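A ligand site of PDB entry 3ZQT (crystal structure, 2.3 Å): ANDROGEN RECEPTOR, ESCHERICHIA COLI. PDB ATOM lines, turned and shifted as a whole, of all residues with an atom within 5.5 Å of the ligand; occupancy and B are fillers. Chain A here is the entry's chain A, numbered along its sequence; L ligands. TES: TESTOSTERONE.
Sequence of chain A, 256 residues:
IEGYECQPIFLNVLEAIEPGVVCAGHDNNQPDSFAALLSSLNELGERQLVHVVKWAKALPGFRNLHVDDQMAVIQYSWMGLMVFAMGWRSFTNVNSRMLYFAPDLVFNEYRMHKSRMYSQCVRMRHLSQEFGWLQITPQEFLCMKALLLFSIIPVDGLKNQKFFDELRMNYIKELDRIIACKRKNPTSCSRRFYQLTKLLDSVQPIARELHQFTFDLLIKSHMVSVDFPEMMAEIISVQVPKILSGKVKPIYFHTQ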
ATOM      1  N   LEU A  38     -10.339   0.144  12.662  1.00  0.00           N
ATOM      2  CA  LEU A  38     -11.233  -0.948  13.028  1.00  0.00           C
ATOM      3  C   LEU A  38     -12.634  -0.481  13.400  1.00  0.00           C
ATOM      4  O   LEU A  38     -13.621  -1.093  13.001  1.00  0.00           O
ATOM      5  CB  LEU A  38     -10.599  -1.875  14.086  1.00  0.00           C
ATOM      6  CG  LEU A  38      -9.747  -3.062  13.577  1.00  0.00           C
ATOM      7  CD1 LEU A  38     -10.625  -4.114  12.823  1.00  0.00           C
ATOM      8  CD2 LEU A  38      -8.584  -2.636  12.697  1.00  0.00           C
ATOM      9  N   LEU A  41     -14.076   0.026   9.981  1.00  0.00           N
ATOM     10  CA  LEU A  41     -14.475  -1.318   9.447  1.00  0.00           C
ATOM     11  C   LEU A  41     -15.707  -1.886  10.139  1.00  0.00           C
ATOM     12  O   LEU A  41     -16.578  -2.459   9.490  1.00  0.00           O
ATOM     13  CB  LEU A  41     -13.334  -2.330   9.542  1.00  0.00           C
ATOM     14  CG  LEU A  41     -12.217  -2.165   8.485  1.00  0.00           C
ATOM     15  CD1 LEU A  41     -11.136  -3.204   8.761  1.00  0.00           C
ATOM     16  CD2 LEU A  41     -12.674  -2.286   7.001  1.00  0.00           C
ATOM     17  N   ASN A  42     -15.775  -1.706  11.459  1.00  0.00           N
ATOM     18  CA  ASN A  42     -16.960  -2.103  12.227  1.00  0.00           C
ATOM     19  C   ASN A  42     -18.227  -1.364  11.876  1.00  0.00           C
ATOM     20  O   ASN A  42     -19.271  -2.004  11.701  1.00  0.00           O
ATOM     21  CB  ASN A  42     -16.723  -1.975  13.736  1.00  0.00           C
ATOM     22  CG  ASN A  42     -15.818  -3.076  14.280  1.00  0.00           C
ATOM     23  OD1 ASN A  42     -15.606  -4.117  13.632  1.00  0.00           O
ATOM     24  ND2 ASN A  42     -15.284  -2.852  15.490  1.00  0.00           N
ATOM     25  N   LEU A  44     -18.692   0.075   9.096  1.00  0.00           N
ATOM     26  CA  LEU A  44     -18.893  -0.445   7.756  1.00  0.00           C
ATOM     27  C   LEU A  44     -19.662  -1.773   7.699  1.00  0.00           C
ATOM     28  O   LEU A  44     -20.459  -1.986   6.779  1.00  0.00           O
ATOM     29  CB  LEU A  44     -17.570  -0.593   6.998  1.00  0.00           C
ATOM     30  CG  LEU A  44     -17.800  -1.049   5.534  1.00  0.00           C
ATOM     31  CD1 LEU A  44     -18.823  -0.115   4.748  1.00  0.00           C
ATOM     32  CD2 LEU A  44     -16.523  -1.168   4.730  1.00  0.00           C
ATOM     33  N   GLY A  45     -19.395  -2.651   8.680  1.00  0.00           N
ATOM     34  CA  GLY A  45     -20.117  -3.900   8.811  1.00  0.00           C
ATOM     35  C   GLY A  45     -21.574  -3.676   9.134  1.00  0.00           C
ATOM     36  O   GLY A  45     -22.439  -4.242   8.485  1.00  0.00           O
ATOM     37  N   GLN A  48     -23.200  -2.356   5.904  1.00  0.00           N
ATOM     38  CA  GLN A  48     -23.328  -3.393   4.878  1.00  0.00           C
ATOM     39  C   GLN A  48     -24.433  -4.404   5.227  1.00  0.00           C
ATOM     40  O   GLN A  48     -25.054  -4.986   4.345  1.00  0.00           O
ATOM     41  CB  GLN A  48     -22.003  -4.125   4.700  1.00  0.00           C
ATOM     42  CG  GLN A  48     -20.907  -3.274   4.129  1.00  0.00           C
ATOM     43  CD  GLN A  48     -20.886  -3.293   2.623  1.00  0.00           C
ATOM     44  OE1 GLN A  48     -19.964  -2.752   2.005  1.00  0.00           O
ATOM     45  NE2 GLN A  48     -21.893  -3.926   2.012  1.00  0.00           N
ATOM     46  N   TRP A  78     -22.618 -13.719   6.655  1.00  0.00           N
ATOM     47  CA  TRP A  78     -22.331 -12.355   6.205  1.00  0.00           C
ATOM     48  C   TRP A  78     -20.866 -12.105   5.938  1.00  0.00           C
ATOM     49  O   TRP A  78     -20.537 -11.406   4.999  1.00  0.00           O
ATOM     50  CB  TRP A  78     -22.827 -11.337   7.181  1.00  0.00           C
ATOM     51  CG  TRP A  78     -22.359 -11.628   8.565  1.00  0.00           C
ATOM     52  CD1 TRP A  78     -22.893 -12.553   9.410  1.00  0.00           C
ATOM     53  CD2 TRP A  78     -21.259 -11.040   9.246  1.00  0.00           C
ATOM     54  NE1 TRP A  78     -22.194 -12.564  10.589  1.00  0.00           N
ATOM     55  CE2 TRP A  78     -21.181 -11.642  10.523  1.00  0.00           C
ATOM     56  CE3 TRP A  78     -20.326 -10.041   8.911  1.00  0.00           C
ATOM     57  CZ2 TRP A  78     -20.206 -11.294  11.473  1.00  0.00           C
ATOM     58  CZ3 TRP A  78     -19.360  -9.683   9.861  1.00  0.00           C
ATOM     59  CH2 TRP A  78     -19.316 -10.309  11.133  1.00  0.00           C
ATOM     60  N   MET A  79     -19.976 -12.682   6.746  1.00  0.00           N
ATOM     61  CA  MET A  79     -18.537 -12.468   6.594  1.00  0.00           C
ATOM     62  C   MET A  79     -18.114 -12.848   5.200  1.00  0.00           C
ATOM     63  O   MET A  79     -17.597 -11.999   4.462  1.00  0.00           O
ATOM     64  CB  MET A  79     -17.672 -13.231   7.614  1.00  0.00           C
ATOM     65  CG  MET A  79     -16.186 -12.815   7.624  1.00  0.00           C
ATOM     66  SD  MET A  79     -15.927 -11.133   8.202  1.00  0.00           S
ATOM     67  CE  MET A  79     -16.117 -11.409   9.987  1.00  0.00           C
ATOM     68  N   MET A  82     -19.677 -10.579   2.362  1.00  0.00           N
ATOM     69  CA  MET A  82     -19.040  -9.270   2.288  1.00  0.00           C
ATOM     70  C   MET A  82     -17.576  -9.326   1.845  1.00  0.00           C
ATOM     71  O   MET A  82     -17.116  -8.463   1.091  1.00  0.00           O
ATOM     72  CB  MET A  82     -19.143  -8.563   3.618  1.00  0.00           C
ATOM     73  CG  MET A  82     -20.604  -8.272   4.042  1.00  0.00           C
ATOM     74  SD  MET A  82     -20.468  -7.448   5.610  1.00  0.00           S
ATOM     75  CE  MET A  82     -22.201  -7.206   6.119  1.00  0.00           C
ATOM     76  N   VAL A  83     -16.836 -10.324   2.319  1.00  0.00           N
ATOM     77  CA  VAL A  83     -15.452 -10.441   1.883  1.00  0.00           C
ATOM     78  C   VAL A  83     -15.362 -10.641   0.362  1.00  0.00           C
ATOM     79  O   VAL A  83     -14.551  -9.994  -0.324  1.00  0.00           O
ATOM     80  CB  VAL A  83     -14.733 -11.544   2.612  1.00  0.00           C
ATOM     81  CG1 VAL A  83     -13.488 -11.997   1.806  1.00  0.00           C
ATOM     82  CG2 VAL A  83     -14.322 -11.047   3.970  1.00  0.00           C
ATOM     83  N   MET A  86     -16.367  -7.427  -1.535  1.00  0.00           N
ATOM     84  CA  MET A  86     -15.235  -6.525  -1.399  1.00  0.00           C
ATOM     85  C   MET A  86     -14.092  -6.928  -2.324  1.00  0.00           C
ATOM     86  O   MET A  86     -13.444  -6.084  -2.902  1.00  0.00           O
ATOM     87  CB  MET A  86     -14.752  -6.504   0.032  1.00  0.00           C
ATOM     88  CG  MET A  86     -13.734  -5.438   0.301  1.00  0.00           C
ATOM     89  SD  MET A  86     -12.063  -6.029  -0.030  1.00  0.00           S
ATOM     90  CE  MET A  86     -11.819  -6.933   1.527  1.00  0.00           C
ATOM     91  N   ARG A  89     -15.134  -5.660  -5.721  1.00  0.00           N
ATOM     92  CA  ARG A  89     -14.982  -4.179  -5.755  1.00  0.00           C
ATOM     93  C   ARG A  89     -13.519  -3.775  -5.871  1.00  0.00           C
ATOM     94  O   ARG A  89     -13.208  -2.709  -6.420  1.00  0.00           O
ATOM     95  CB  ARG A  89     -15.469  -3.514  -4.452  1.00  0.00           C
ATOM     96  CG  ARG A  89     -16.954  -3.455  -4.277  1.00  0.00           C
ATOM     97  CD  ARG A  89     -17.322  -2.442  -3.156  1.00  0.00           C
ATOM     98  NE  ARG A  89     -16.738  -2.711  -1.837  1.00  0.00           N
ATOM     99  CZ  ARG A  89     -17.307  -3.498  -0.916  1.00  0.00           C
ATOM    100  NH1 ARG A  89     -18.481  -4.112  -1.159  1.00  0.00           N
ATOM    101  NH2 ARG A  89     -16.734  -3.666   0.263  1.00  0.00           N
ATOM    102  N   PHE A 101     -12.454  -1.348   0.584  1.00  0.00           N
ATOM    103  CA  PHE A 101     -13.524  -1.665   1.515  1.00  0.00           C
ATOM    104  C   PHE A 101     -14.744  -0.814   1.226  1.00  0.00           C
ATOM    105  O   PHE A 101     -15.818  -1.341   1.026  1.00  0.00           O
ATOM    106  CB  PHE A 101     -13.059  -1.555   2.970  1.00  0.00           C
ATOM    107  CG  PHE A 101     -12.164  -2.654   3.402  1.00  0.00           C
ATOM    108  CD1 PHE A 101     -12.696  -3.889   3.823  1.00  0.00           C
ATOM    109  CD2 PHE A 101     -10.781  -2.473   3.424  1.00  0.00           C
ATOM    110  CE1 PHE A 101     -11.888  -4.916   4.249  1.00  0.00           C
ATOM    111  CE2 PHE A 101      -9.904  -3.540   3.850  1.00  0.00           C
ATOM    112  CZ  PHE A 101     -10.473  -4.752   4.275  1.00  0.00           C
ATOM    113  N   MET A 117      -3.989  -6.648  10.542  1.00  0.00           N
ATOM    114  CA  MET A 117      -4.452  -7.865   9.887  1.00  0.00           C
ATOM    115  C   MET A 117      -3.718  -8.083   8.599  1.00  0.00           C
ATOM    116  O   MET A 117      -4.289  -8.565   7.616  1.00  0.00           O
ATOM    117  CB  MET A 117      -5.936  -7.823   9.607  1.00  0.00           C
ATOM    118  CG  MET A 117      -6.718  -6.905  10.518  1.00  0.00           C
ATOM    119  SD  MET A 117      -8.439  -7.075  10.062  1.00  0.00           S
ATOM    120  CE  MET A 117      -8.512  -6.067   8.593  1.00  0.00           C
ATOM    121  N   MET A 124      -7.101 -11.854   1.619  1.00  0.00           N
ATOM    122  CA  MET A 124      -8.202 -11.159   0.942  1.00  0.00           C
ATOM    123  C   MET A 124      -7.826 -10.575  -0.413  1.00  0.00           C
ATOM    124  O   MET A 124      -8.659 -10.554  -1.319  1.00  0.00           O
ATOM    125  CB  MET A 124      -8.792 -10.067   1.826  1.00  0.00           C
ATOM    126  CG  MET A 124      -9.716 -10.591   2.899  1.00  0.00           C
ATOM    127  SD  MET A 124     -10.489  -9.233   3.809  1.00  0.00           S
ATOM    128  CE  MET A 124      -9.232  -8.742   4.965  1.00  0.00           C
ATOM    129  N   LEU A 210     -11.381 -14.375   9.857  1.00  0.00           N
ATOM    130  CA  LEU A 210     -11.866 -13.039  10.233  1.00  0.00           C
ATOM    131  C   LEU A 210     -12.799 -13.169  11.390  1.00  0.00           C
ATOM    132  O   LEU A 210     -12.946 -12.267  12.194  1.00  0.00           O
ATOM    133  CB  LEU A 210     -12.507 -12.297   9.038  1.00  0.00           C
ATOM    134  CG  LEU A 210     -11.480 -12.175   7.902  1.00  0.00           C
ATOM    135  CD1 LEU A 210     -12.087 -12.183   6.524  1.00  0.00           C
ATOM    136  CD2 LEU A 210     -10.582 -10.968   8.076  1.00  0.00           C
ATOM    137  N   PHE A 213     -10.357 -13.355  14.366  1.00  0.00           N
ATOM    138  CA  PHE A 213      -9.870 -11.992  14.581  1.00  0.00           C
ATOM    139  C   PHE A 213     -10.899 -11.112  15.277  1.00  0.00           C
ATOM    140  O   PHE A 213     -10.655 -10.649  16.386  1.00  0.00           O
ATOM    141  CB  PHE A 213      -9.438 -11.348  13.287  1.00  0.00           C
ATOM    142  CG  PHE A 213      -8.551 -10.156  13.489  1.00  0.00           C
ATOM    143  CD1 PHE A 213      -9.091  -8.902  13.727  1.00  0.00           C
ATOM    144  CD2 PHE A 213      -7.157 -10.312  13.484  1.00  0.00           C
ATOM    145  CE1 PHE A 213      -8.272  -7.810  13.955  1.00  0.00           C
ATOM    146  CE2 PHE A 213      -6.325  -9.247  13.710  1.00  0.00           C
ATOM    147  CZ  PHE A 213      -6.870  -7.988  13.941  1.00  0.00           C
ATOM    148  N   THR A 214     -12.064 -10.928  14.655  1.00  0.00           N
ATOM    149  CA  THR A 214     -13.048  -9.976  15.171  1.00  0.00           C
ATOM    150  C   THR A 214     -13.638 -10.433  16.531  1.00  0.00           C
ATOM    151  O   THR A 214     -13.954  -9.627  17.404  1.00  0.00           O
ATOM    152  CB  THR A 214     -14.156  -9.735  14.120  1.00  0.00           C
ATOM    153  OG1 THR A 214     -14.996  -8.638  14.520  1.00  0.00           O
ATOM    154  CG2 THR A 214     -15.047 -11.005  13.952  1.00  0.00           C
ATOM    155  N   LEU A 217     -11.107  -9.437  18.885  1.00  0.00           N
ATOM    156  CA  LEU A 217     -11.156  -8.000  18.988  1.00  0.00           C
ATOM    157  C   LEU A 217     -12.309  -7.534  19.893  1.00  0.00           C
ATOM    158  O   LEU A 217     -12.148  -6.668  20.730  1.00  0.00           O
ATOM    159  CB  LEU A 217     -11.278  -7.420  17.580  1.00  0.00           C
ATOM    160  CG  LEU A 217     -11.292  -5.898  17.368  1.00  0.00           C
ATOM    161  CD1 LEU A 217     -10.262  -5.227  18.247  1.00  0.00           C
ATOM    162  CD2 LEU A 217     -10.954  -5.564  15.913  1.00  0.00           C
ATOM    163  N   PHE A 228     -17.818  -1.282  18.655  1.00  0.00           N
ATOM    164  CA  PHE A 228     -18.631  -2.188  17.883  1.00  0.00           C
ATOM    165  C   PHE A 228     -20.063  -1.694  17.967  1.00  0.00           C
ATOM    166  O   PHE A 228     -20.611  -1.574  19.069  1.00  0.00           O
ATOM    167  CB  PHE A 228     -18.537  -3.599  18.430  1.00  0.00           C
ATOM    168  CG  PHE A 228     -17.279  -4.349  18.037  1.00  0.00           C
ATOM    169  CD1 PHE A 228     -16.063  -4.090  18.669  1.00  0.00           C
ATOM    170  CD2 PHE A 228     -17.331  -5.345  17.070  1.00  0.00           C
ATOM    171  CE1 PHE A 228     -14.913  -4.801  18.321  1.00  0.00           C
ATOM    172  CE2 PHE A 228     -16.185  -6.067  16.700  1.00  0.00           C
ATOM    173  CZ  PHE A 228     -14.973  -5.804  17.339  1.00  0.00           C
ATOM    174  N   MET A 232     -23.377  -5.618  15.214  1.00  0.00           N
ATOM    175  CA  MET A 232     -22.083  -6.274  15.075  1.00  0.00           C
ATOM    176  C   MET A 232     -21.687  -6.921  16.382  1.00  0.00           C
ATOM    177  O   MET A 232     -21.209  -8.029  16.386  1.00  0.00           O
ATOM    178  CB  MET A 232     -20.992  -5.281  14.663  1.00  0.00           C
ATOM    179  CG  MET A 232     -21.132  -4.739  13.255  1.00  0.00           C
ATOM    180  SD  MET A 232     -20.867  -6.000  11.968  1.00  0.00           S
ATOM    181  CE  MET A 232     -19.103  -5.858  11.775  1.00  0.00           C
ATOM    182  N   ILE A 236     -21.503 -10.989  16.658  1.00  0.00           N
ATOM    183  CA  ILE A 236     -20.214 -11.529  16.946  1.00  0.00           C
ATOM    184  C   ILE A 236     -20.164 -12.267  18.294  1.00  0.00           C
ATOM    185  O   ILE A 236     -19.386 -13.197  18.454  1.00  0.00           O
ATOM    186  CB  ILE A 236     -19.182 -10.432  16.817  1.00  0.00           C
ATOM    187  CG1 ILE A 236     -19.036 -10.153  15.284  1.00  0.00           C
ATOM    188  CG2 ILE A 236     -17.895 -10.814  17.547  1.00  0.00           C
ATOM    189  CD1 ILE A 236     -18.659  -8.705  14.899  1.00  0.00           C
HETATM  190  C1  TES L   1     -16.670  -4.999   6.226  1.00  0.00           C
HETATM  191  C2  TES L   1     -17.291  -4.951   4.843  1.00  0.00           C
HETATM  192  C3  TES L   1     -16.288  -5.500   3.863  1.00  0.00           C
HETATM  193  O3  TES L   1     -16.267  -5.072   2.718  1.00  0.00           O
HETATM  194  C4  TES L   1     -15.317  -6.533   4.283  1.00  0.00           C
HETATM  195  C5  TES L   1     -15.177  -6.914   5.571  1.00  0.00           C
HETATM  196  C6  TES L   1     -14.045  -7.887   5.916  1.00  0.00           C
HETATM  197  C7  TES L   1     -13.329  -7.417   7.178  1.00  0.00           C
HETATM  198  C8  TES L   1     -14.323  -7.246   8.330  1.00  0.00           C
HETATM  199  C9  TES L   1     -15.402  -6.199   7.983  1.00  0.00           C
HETATM  200  C10 TES L   1     -16.113  -6.385   6.631  1.00  0.00           C
HETATM  201  C11 TES L   1     -16.380  -5.961   9.127  1.00  0.00           C
HETATM  202  C12 TES L   1     -15.572  -5.486  10.361  1.00  0.00           C
HETATM  203  C13 TES L   1     -14.561  -6.559  10.777  1.00  0.00           C
HETATM  204  C14 TES L   1     -13.613  -6.783   9.607  1.00  0.00           C
HETATM  205  C15 TES L   1     -12.509  -7.686  10.182  1.00  0.00           C
HETATM  206  C16 TES L   1     -12.438  -7.281  11.664  1.00  0.00           C
HETATM  207  C17 TES L   1     -13.570  -6.271  11.909  1.00  0.00           C
HETATM  208  O17 TES L   1     -14.058  -6.463  13.250  1.00  0.00           O
HETATM  209  C18 TES L   1     -15.314  -7.831  11.159  1.00  0.00           C
HETATM  210  C19 TES L   1     -17.253  -7.418   6.735  1.00  0.00           C
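O of Leu 38 sits close to ND2 of Asn 42, 3.5 Å away.
The guanidinium group of Arg 89 lies within hydrogen-bond range of the backbone carbonyl oxygen of Phe 101, 2.6 Å away.
Leu 38 touches the ligand.
Leu 41 touches the ligand (O to C12, 3.3 Å).
Leu 44 touches the ligand.
Met 79 touches the ligand.
SD of Met 82 touches C19 of the ligand (3.4 Å).
Val 83 touches the ligand.
CB of Met 86 touches O3 of the ligand, at 3.4 Å.
Phe 101 touches the ligand.
Met 232 touches the ligand (CE to C11, 3.8 Å).
Hydrophobic or aromatic side chains that line the ligand: Leu 38, Leu 41, Leu 44, Met 79, Met 82, Val 83, Met 86, Phe 101 and Met 232.
12 residues have an atom within 4 Å of the ligand: Leu 38, Leu 41, Asn 42, Leu 44, Met 79, Met 82, Val 83, Met 86, Arg 89, Phe 101, Thr 214 and Met 232.
Along chain A the residues within 4 Å of the ligand span positions 38 to 232.
NH2 of Arg 89 sits at hydrogen-bond distance from O3 of the ligand.
O17 of the ligand sits at hydrogen-bond distance from OG1 of Thr 214.
The side-chain amide oxygen (OD1) of Asn 42 sits at hydrogen-bond distance from an oxygen (O17) of the ligand (2.8 Å).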
